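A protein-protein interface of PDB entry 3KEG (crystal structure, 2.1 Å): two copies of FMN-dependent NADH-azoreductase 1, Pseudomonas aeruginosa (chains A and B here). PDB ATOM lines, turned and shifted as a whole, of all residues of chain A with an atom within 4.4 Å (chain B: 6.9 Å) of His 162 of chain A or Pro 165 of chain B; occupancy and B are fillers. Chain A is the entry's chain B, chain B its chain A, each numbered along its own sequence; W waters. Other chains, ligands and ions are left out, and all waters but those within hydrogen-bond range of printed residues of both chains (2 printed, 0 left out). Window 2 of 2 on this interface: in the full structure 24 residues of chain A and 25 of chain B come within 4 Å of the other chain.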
ATOM      1  N   PHE A 100       5.193  24.530  19.165  1.00  0.00           N
ATOM      2  CA  PHE A 100       5.555  23.205  19.666  1.00  0.00           C
ATOM      3  C   PHE A 100       6.934  22.738  19.202  1.00  0.00           C
ATOM      4  O   PHE A 100       7.286  21.570  19.358  1.00  0.00           O
ATOM      5  CB  PHE A 100       4.477  22.194  19.275  1.00  0.00           C
ATOM      6  CG  PHE A 100       3.086  22.655  19.594  1.00  0.00           C
ATOM      7  CD1 PHE A 100       2.628  22.656  20.902  1.00  0.00           C
ATOM      8  CD2 PHE A 100       2.242  23.106  18.592  1.00  0.00           C
ATOM      9  CE1 PHE A 100       1.350  23.088  21.203  1.00  0.00           C
ATOM     10  CE2 PHE A 100       0.964  23.539  18.886  1.00  0.00           C
ATOM     11  CZ  PHE A 100       0.518  23.530  20.194  1.00  0.00           C
ATOM     12  N   SER A 101       7.711  23.656  18.639  1.00  0.00           N
ATOM     13  CA  SER A 101       9.096  23.382  18.270  1.00  0.00           C
ATOM     14  C   SER A 101       9.928  24.637  18.541  1.00  0.00           C
ATOM     15  O   SER A 101       9.564  25.446  19.391  1.00  0.00           O
ATOM     16  CB  SER A 101       9.184  22.956  16.801  1.00  0.00           C
ATOM     17  OG  SER A 101      10.487  22.513  16.464  1.00  0.00           O
ATOM     18  N   ALA A 159       3.700  15.457  25.613  1.00  0.00           N
ATOM     19  CA  ALA A 159       3.868  14.792  24.323  1.00  0.00           C
ATOM     20  C   ALA A 159       3.851  15.779  23.157  1.00  0.00           C
ATOM     21  O   ALA A 159       4.272  15.446  22.051  1.00  0.00           O
ATOM     22  CB  ALA A 159       2.793  13.726  24.131  1.00  0.00           C
ATOM     23  N   MET A 160       3.361  16.990  23.403  1.00  0.00           N
ATOM     24  CA  MET A 160       3.326  18.019  22.369  1.00  0.00           C
ATOM     25  C   MET A 160       4.662  18.747  22.243  1.00  0.00           C
ATOM     26  O   MET A 160       4.880  19.490  21.287  1.00  0.00           O
ATOM     27  CB  MET A 160       2.236  19.050  22.671  1.00  0.00           C
ATOM     28  CG  MET A 160       0.841  18.479  22.854  1.00  0.00           C
ATOM     29  SD  MET A 160      -0.374  19.803  23.015  1.00  0.00           S
ATOM     30  CE  MET A 160      -1.779  18.920  23.687  1.00  0.00           C
ATOM     31  N   ASN A 161       5.553  18.540  23.207  1.00  0.00           N
ATOM     32  CA  ASN A 161       6.812  19.278  23.242  1.00  0.00           C
ATOM     33  C   ASN A 161       7.851  18.712  22.285  1.00  0.00           C
ATOM     34  O   ASN A 161       8.493  17.701  22.573  1.00  0.00           O
ATOM     35  CB  ASN A 161       7.383  19.310  24.661  1.00  0.00           C
ATOM     36  CG  ASN A 161       8.510  20.315  24.810  1.00  0.00           C
ATOM     37  OD1 ASN A 161       9.014  20.850  23.824  1.00  0.00           O
ATOM     38  ND2 ASN A 161       8.907  20.581  26.046  1.00  0.00           N
ATOM     39  N   HIS A 162       8.014  19.377  21.148  1.00  0.00           N
ATOM     40  CA  HIS A 162       9.010  18.987  20.160  1.00  0.00           C
ATOM     41  C   HIS A 162      10.093  20.064  20.033  1.00  0.00           C
ATOM     42  O   HIS A 162      10.751  20.179  19.000  1.00  0.00           O
ATOM     43  CB  HIS A 162       8.344  18.732  18.802  1.00  0.00           C
ATOM     44  CG  HIS A 162       7.336  17.622  18.814  1.00  0.00           C
ATOM     45  ND1 HIS A 162       7.690  16.294  18.729  1.00  0.00           N
ATOM     46  CD2 HIS A 162       5.983  17.641  18.885  1.00  0.00           C
ATOM     47  CE1 HIS A 162       6.606  15.541  18.756  1.00  0.00           C
ATOM     48  NE2 HIS A 162       5.555  16.335  18.849  1.00  0.00           N
ATOM     49  N   ALA A 163      10.268  20.847  21.094  1.00  0.00           N
ATOM     50  CA  ALA A 163      11.280  21.900  21.121  1.00  0.00           C
ATOM     51  C   ALA A 163      12.564  21.418  21.797  1.00  0.00           C
ATOM     52  O   ALA A 163      13.507  21.016  21.118  1.00  0.00           O
ATOM     53  CB  ALA A 163      10.737  23.150  21.818  1.00  0.00           C
ATOM     54  N   ASP A 164      12.606  21.450  23.128  1.00  0.00           N
ATOM     55  CA  ASP A 164      13.831  21.083  23.844  1.00  0.00           C
ATOM     56  C   ASP A 164      14.098  19.575  23.857  1.00  0.00           C
ATOM     57  O   ASP A 164      15.256  19.159  23.892  1.00  0.00           O
ATOM     58  CB  ASP A 164      13.850  21.648  25.272  1.00  0.00           C
ATOM     59  CG  ASP A 164      12.580  21.355  26.040  1.00  0.00           C
ATOM     60  OD1 ASP A 164      11.620  22.142  25.913  1.00  0.00           O
ATOM     61  OD2 ASP A 164      12.544  20.346  26.775  1.00  0.00           O
ATOM     62  N   TRP A 166      13.572  17.673  21.325  1.00  0.00           N
ATOM     63  CA  TRP A 166      14.180  17.450  20.021  1.00  0.00           C
ATOM     64  C   TRP A 166      15.621  17.955  19.998  1.00  0.00           C
ATOM     65  O   TRP A 166      16.485  17.347  19.367  1.00  0.00           O
ATOM     66  CB  TRP A 166      13.393  18.129  18.904  1.00  0.00           C
ATOM     67  CG  TRP A 166      14.238  18.300  17.694  1.00  0.00           C
ATOM     68  CD1 TRP A 166      14.548  17.345  16.773  1.00  0.00           C
ATOM     69  CD2 TRP A 166      14.929  19.491  17.289  1.00  0.00           C
ATOM     70  NE1 TRP A 166      15.375  17.871  15.811  1.00  0.00           N
ATOM     71  CE2 TRP A 166      15.622  19.180  16.104  1.00  0.00           C
ATOM     72  CE3 TRP A 166      15.017  20.783  17.810  1.00  0.00           C
ATOM     73  CZ2 TRP A 166      16.396  20.124  15.430  1.00  0.00           C
ATOM     74  CZ3 TRP A 166      15.786  21.715  17.139  1.00  0.00           C
ATOM     75  CH2 TRP A 166      16.464  21.381  15.960  1.00  0.00           C
ATOM     76  N   MET B  97      13.535  14.135   6.428  1.00  0.00           N
ATOM     77  CA  MET B  97      13.877  14.295   7.830  1.00  0.00           C
ATOM     78  C   MET B  97      15.276  14.884   7.898  1.00  0.00           C
ATOM     79  O   MET B  97      16.244  14.262   7.461  1.00  0.00           O
ATOM     80  CB  MET B  97      13.830  12.970   8.589  1.00  0.00           C
ATOM     81  CG  MET B  97      14.480  13.061   9.962  1.00  0.00           C
ATOM     82  SD  MET B  97      14.400  11.532  10.911  1.00  0.00           S
ATOM     83  CE  MET B  97      12.713  11.584  11.509  1.00  0.00           C
ATOM     84  N   SER B 101      14.145  16.293  12.582  1.00  0.00           N
ATOM     85  CA  SER B 101      13.007  17.192  12.436  1.00  0.00           C
ATOM     86  C   SER B 101      12.807  17.484  10.948  1.00  0.00           C
ATOM     87  O   SER B 101      13.178  16.671  10.104  1.00  0.00           O
ATOM     88  CB  SER B 101      13.232  18.479  13.235  1.00  0.00           C
ATOM     89  OG  SER B 101      12.063  19.279  13.268  1.00  0.00           O
ATOM     90  N   ILE B 142       1.151  13.574   4.556  1.00  0.00           N
ATOM     91  CA  ILE B 142       2.563  13.884   4.718  1.00  0.00           C
ATOM     92  C   ILE B 142       3.406  12.813   4.048  1.00  0.00           C
ATOM     93  O   ILE B 142       3.367  11.649   4.432  1.00  0.00           O
ATOM     94  CB  ILE B 142       2.959  13.966   6.201  1.00  0.00           C
ATOM     95  CG1 ILE B 142       2.196  15.100   6.890  1.00  0.00           C
ATOM     96  CG2 ILE B 142       4.458  14.179   6.333  1.00  0.00           C
ATOM     97  CD1 ILE B 142       2.495  15.232   8.370  1.00  0.00           C
ATOM     98  N   ARG B 146      13.505   9.423   4.673  1.00  0.00           N
ATOM     99  CA  ARG B 146      14.544   9.456   5.688  1.00  0.00           C
ATOM    100  C   ARG B 146      15.713   8.598   5.231  1.00  0.00           C
ATOM    101  O   ARG B 146      15.524   7.596   4.545  1.00  0.00           O
ATOM    102  CB  ARG B 146      14.006   8.912   7.009  1.00  0.00           C
ATOM    103  CG  ARG B 146      12.697   9.532   7.453  1.00  0.00           C
ATOM    104  CD  ARG B 146      12.027   8.659   8.493  1.00  0.00           C
ATOM    105  NE  ARG B 146      10.695   9.140   8.841  1.00  0.00           N
ATOM    106  CZ  ARG B 146       9.666   8.353   9.137  1.00  0.00           C
ATOM    107  NH1 ARG B 146       9.803   7.036   9.124  1.00  0.00           N
ATOM    108  NH2 ARG B 146       8.491   8.883   9.441  1.00  0.00           N
ATOM    109  N   PHE B 151      12.066   4.979  12.224  1.00  0.00           N
ATOM    110  CA  PHE B 151      11.542   6.216  12.793  1.00  0.00           C
ATOM    111  C   PHE B 151      10.014   6.231  12.808  1.00  0.00           C
ATOM    112  O   PHE B 151       9.403   7.133  13.375  1.00  0.00           O
ATOM    113  CB  PHE B 151      12.081   7.424  12.025  1.00  0.00           C
ATOM    114  CG  PHE B 151      13.542   7.682  12.257  1.00  0.00           C
ATOM    115  CD1 PHE B 151      13.973   8.292  13.425  1.00  0.00           C
ATOM    116  CD2 PHE B 151      14.485   7.319  11.309  1.00  0.00           C
ATOM    117  CE1 PHE B 151      15.316   8.532  13.644  1.00  0.00           C
ATOM    118  CE2 PHE B 151      15.832   7.557  11.523  1.00  0.00           C
ATOM    119  CZ  PHE B 151      16.247   8.164  12.691  1.00  0.00           C
ATOM    120  N   GLN B 158      11.643   5.426  17.010  1.00  0.00           N
ATOM    121  CA  GLN B 158      10.439   6.245  16.906  1.00  0.00           C
ATOM    122  C   GLN B 158      10.472   7.481  17.810  1.00  0.00           C
ATOM    123  O   GLN B 158       9.917   8.523  17.461  1.00  0.00           O
ATOM    124  CB  GLN B 158       9.206   5.406  17.235  1.00  0.00           C
ATOM    125  CG  GLN B 158       7.898   6.124  16.984  1.00  0.00           C
ATOM    126  CD  GLN B 158       6.708   5.375  17.544  1.00  0.00           C
ATOM    127  OE1 GLN B 158       6.853   4.293  18.113  1.00  0.00           O
ATOM    128  NE2 GLN B 158       5.522   5.947  17.388  1.00  0.00           N
ATOM    129  N   ASN B 161      11.948  10.700  16.408  1.00  0.00           N
ATOM    130  CA  ASN B 161      11.257  11.343  15.296  1.00  0.00           C
ATOM    131  C   ASN B 161      10.461  12.566  15.731  1.00  0.00           C
ATOM    132  O   ASN B 161       9.385  12.444  16.317  1.00  0.00           O
ATOM    133  CB  ASN B 161      10.327  10.351  14.597  1.00  0.00           C
ATOM    134  CG  ASN B 161       9.746  10.909  13.310  1.00  0.00           C
ATOM    135  OD1 ASN B 161       9.907  12.088  13.006  1.00  0.00           O
ATOM    136  ND2 ASN B 161       9.072  10.061  12.548  1.00  0.00           N
ATOM    137  N   HIS B 162      11.002  13.743  15.440  1.00  0.00           N
ATOM    138  CA  HIS B 162      10.315  14.999  15.708  1.00  0.00           C
ATOM    139  C   HIS B 162      10.000  15.727  14.398  1.00  0.00           C
ATOM    140  O   HIS B 162       9.877  16.951  14.368  1.00  0.00           O
ATOM    141  CB  HIS B 162      11.164  15.879  16.631  1.00  0.00           C
ATOM    142  CG  HIS B 162      11.429  15.269  17.974  1.00  0.00           C
ATOM    143  ND1 HIS B 162      10.556  15.397  19.033  1.00  0.00           N
ATOM    144  CD2 HIS B 162      12.465  14.527  18.436  1.00  0.00           C
ATOM    145  CE1 HIS B 162      11.039  14.764  20.084  1.00  0.00           C
ATOM    146  NE2 HIS B 162      12.194  14.228  19.749  1.00  0.00           N
ATOM    147  N   ALA B 163       9.873  14.957  13.321  1.00  0.00           N
ATOM    148  CA  ALA B 163       9.547  15.494  12.003  1.00  0.00           C
ATOM    149  C   ALA B 163       8.039  15.446  11.745  1.00  0.00           C
ATOM    150  O   ALA B 163       7.347  16.444  11.937  1.00  0.00           O
ATOM    151  CB  ALA B 163      10.305  14.731  10.915  1.00  0.00           C
ATOM    152  N   ASP B 164       7.528  14.295  11.313  1.00  0.00           N
ATOM    153  CA  ASP B 164       6.100  14.179  11.002  1.00  0.00           C
ATOM    154  C   ASP B 164       5.228  14.111  12.259  1.00  0.00           C
ATOM    155  O   ASP B 164       4.095  14.589  12.245  1.00  0.00           O
ATOM    156  CB  ASP B 164       5.802  12.991  10.072  1.00  0.00           C
ATOM    157  CG  ASP B 164       6.491  11.717  10.503  1.00  0.00           C
ATOM    158  OD1 ASP B 164       7.700  11.581  10.229  1.00  0.00           O
ATOM    159  OD2 ASP B 164       5.824  10.846  11.100  1.00  0.00           O
ATOM    160  N   PRO B 165       5.740  13.515  13.348  1.00  0.00           N
ATOM    161  CA  PRO B 165       4.927  13.572  14.567  1.00  0.00           C
ATOM    162  C   PRO B 165       4.742  14.998  15.077  1.00  0.00           C
ATOM    163  O   PRO B 165       3.681  15.312  15.616  1.00  0.00           O
ATOM    164  CB  PRO B 165       5.732  12.739  15.568  1.00  0.00           C
ATOM    165  CG  PRO B 165       6.527  11.814  14.724  1.00  0.00           C
ATOM    166  CD  PRO B 165       6.898  12.621  13.513  1.00  0.00           C
ATOM    167  N   TRP B 166       5.752  15.847  14.917  1.00  0.00           N
ATOM    168  CA  TRP B 166       5.598  17.246  15.290  1.00  0.00           C
ATOM    169  C   TRP B 166       4.620  17.946  14.352  1.00  0.00           C
ATOM    170  O   TRP B 166       3.822  18.774  14.785  1.00  0.00           O
ATOM    171  CB  TRP B 166       6.926  17.998  15.274  1.00  0.00           C
ATOM    172  CG  TRP B 166       6.695  19.468  15.201  1.00  0.00           C
ATOM    173  CD1 TRP B 166       6.286  20.280  16.217  1.00  0.00           C
ATOM    174  CD2 TRP B 166       6.808  20.300  14.043  1.00  0.00           C
ATOM    175  NE1 TRP B 166       6.156  21.569  15.768  1.00  0.00           N
ATOM    176  CE2 TRP B 166       6.472  21.610  14.433  1.00  0.00           C
ATOM    177  CE3 TRP B 166       7.174  20.068  12.712  1.00  0.00           C
ATOM    178  CZ2 TRP B 166       6.487  22.684  13.548  1.00  0.00           C
ATOM    179  CZ3 TRP B 166       7.189  21.136  11.832  1.00  0.00           C
ATOM    180  CH2 TRP B 166       6.848  22.426  12.255  1.00  0.00           C
ATOM    181  N   LEU B 167       4.693  17.622  13.065  1.00  0.00           N
ATOM    182  CA  LEU B 167       3.777  18.201  12.089  1.00  0.00           C
ATOM    183  C   LEU B 167       2.337  17.883  12.468  1.00  0.00           C
ATOM    184  O   LEU B 167       1.452  18.716  12.304  1.00  0.00           O
ATOM    185  CB  LEU B 167       4.074  17.688  10.679  1.00  0.00           C
ATOM    186  CG  LEU B 167       5.213  18.386   9.929  1.00  0.00           C
ATOM    187  CD1 LEU B 167       5.565  17.629   8.658  1.00  0.00           C
ATOM    188  CD2 LEU B 167       4.842  19.828   9.606  1.00  0.00           C
ATOM    189  N   ARG B 168       2.108  16.675  12.974  1.00  0.00           N
ATOM    190  CA  ARG B 168       0.781  16.281  13.431  1.00  0.00           C
ATOM    191  C   ARG B 168       0.303  17.206  14.540  1.00  0.00           C
ATOM    192  O   ARG B 168      -0.847  17.637  14.547  1.00  0.00           O
ATOM    193  CB  ARG B 168       0.789  14.847  13.956  1.00  0.00           C
ATOM    194  CG  ARG B 168       0.749  13.771  12.889  1.00  0.00           C
ATOM    195  CD  ARG B 168       0.533  12.410  13.527  1.00  0.00           C
ATOM    196  NE  ARG B 168       0.693  11.307  12.584  1.00  0.00           N
ATOM    197  CZ  ARG B 168      -0.296  10.756  11.885  1.00  0.00           C
ATOM    198  NH1 ARG B 168      -0.039   9.754  11.056  1.00  0.00           N
ATOM    199  NH2 ARG B 168      -1.540  11.201  12.011  1.00  0.00           N
ATOM    200  N   THR B 169       1.189  17.494  15.488  1.00  0.00           N
ATOM    201  CA  THR B 169       0.845  18.334  16.629  1.00  0.00           C
ATOM    202  C   THR B 169       0.474  19.749  16.192  1.00  0.00           C
ATOM    203  O   THR B 169      -0.533  20.296  16.638  1.00  0.00           O
ATOM    204  CB  THR B 169       2.006  18.409  17.643  1.00  0.00           C
ATOM    205  OG1 THR B 169       2.366  17.087  18.064  1.00  0.00           O
ATOM    206  CG2 THR B 169       1.604  19.230  18.859  1.00  0.00           C
ATOM    207  N   ALA B 170       1.287  20.337  15.321  1.00  0.00           N
ATOM    208  CA  ALA B 170       1.060  21.707  14.869  1.00  0.00           C
ATOM    209  C   ALA B 170      -0.185  21.811  13.988  1.00  0.00           C
ATOM    210  O   ALA B 170      -0.980  22.739  14.133  1.00  0.00           O
ATOM    211  CB  ALA B 170       2.285  22.226  14.127  1.00  0.00           C
ATOM    212  N   VAL B 181       0.488   9.627   7.052  1.00  0.00           N
ATOM    213  CA  VAL B 181       1.918   9.718   6.767  1.00  0.00           C
ATOM    214  C   VAL B 181       2.384   8.526   5.938  1.00  0.00           C
ATOM    215  O   VAL B 181       2.178   7.376   6.323  1.00  0.00           O
ATOM    216  CB  VAL B 181       2.757   9.752   8.062  1.00  0.00           C
ATOM    217  CG1 VAL B 181       4.248   9.702   7.739  1.00  0.00           C
ATOM    218  CG2 VAL B 181       2.431  10.986   8.889  1.00  0.00           C
HETATM  219  O   HOH W   1      10.801  19.718  15.529  1.00  0.00           O
HETATM  220  O   HOH W   2       3.359  14.325  19.543  1.00  0.00           O
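A ring nitrogen (ND1) of His 162 of chain A lies within hydrogen-bond range of a ring nitrogen (ND1) of His 162 of chain B (3.0 Å).
OG1 of Thr 169 of chain B lies within hydrogen-bond range of NE2 of His 162 of chain A (3.4 Å).
OG of Ser 101 of chain A is in hydrogen-bond range of O of His 162 of chain A, at 3.5 Å.
OG1 of Thr 169 of chain B lies within hydrogen-bond range of O of Pro 165 of chain B (3.3 Å).
O of His 162 of chain B lies within hydrogen-bond range of OG of Ser 101 of chain B (3.4 Å).
N of His 162 of chain A lies within hydrogen-bond range of O of Phe 100 of chain A, at 2.9 Å.
Trp 166 of chain B touches Phe 100 of chain A (CD1 to O, 3.5 Å).
CG of Phe 100 of chain A touches CG2 of Thr 169 of chain B, at 3.8 Å.
NE1 of Trp 166 of chain B touches CB of Ser 101 of chain A, at 3.5 Å.
CG2 of Thr 169 of chain B touches CB of Met 160 of chain A, at 3.9 Å.
His 162 of chain A touches Pro 165 of chain B.
Trp 166 of chain B touches His 162 of chain A (CB to CG, 3.6 Å).
NE1 of Trp 166 of chain A touches CB of Ser 101 of chain B (3.4 Å).
Trp 166 of chain A touches His 162 of chain B (CB to CG, 3.6 Å).
Of the printed residues of chain B, Ser 101 of chain A touches Trp 166 (3.5 Å).
Pro 165 of chain B touches just one residue of chain A: His 162 (3.9 Å).
Of the printed residues of chain A, Trp 166 of chain B touches Phe 100 (3.5 Å), Ser 101 (3.5 Å) and His 162 (3.6 Å).
Ala 170 of chain B touches none of the printed residues of chain A.
Val 181 of chain B touches none of the printed residues of chain A.
The nearest residue of chain B that does not touch His 162 of chain A is Asn 161 of chain B (4.8 Å).
The nearest printed residue of chain A that does not touch Pro 165 of chain B is Ala 159 of chain A (6.5 Å).
The nearest printed residue of chain A that does not touch Trp 166 of chain B is Met 160 of chain A (5.3 Å).
Of the 9 printed residues of chain A, 5 touch a printed residue of chain B.
Hydrophobic or aromatic side chains of chain A within 4 Å of the printed part of chain B: Phe 100, Met 160, His 162 and Trp 166.
Hydrophobic or aromatic side chains of chain B within 4 Å of the printed part of chain A: His 162 and Trp 166.
Ser 101 of chain A touches Trp 166 of chain B, and with the chains exchanged Trp 166 of chain A touches Ser 101 of chain B.
His 162 of chain A touches its own counterpart, His 162 of chain B.
His 162 of chain A touches Trp 166 of chain B, and with the chains exchanged Trp 166 of chain A touches His 162 of chain B.
6 positions are printed for both chains.
Water W1 lies within hydrogen-bond range of OG of Ser 101 of chain B (2.6 Å), OG of Ser 101 of chain A (3.0 Å) and O of His 162 of chain B (3.1 Å).
Water W2 lies within hydrogen-bond range of O of Ala 159 of chain A (2.9 Å), NE2 of His 162 of chain A (3.1 Å) and OG1 of Thr 169 of chain B (3.3 Å).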
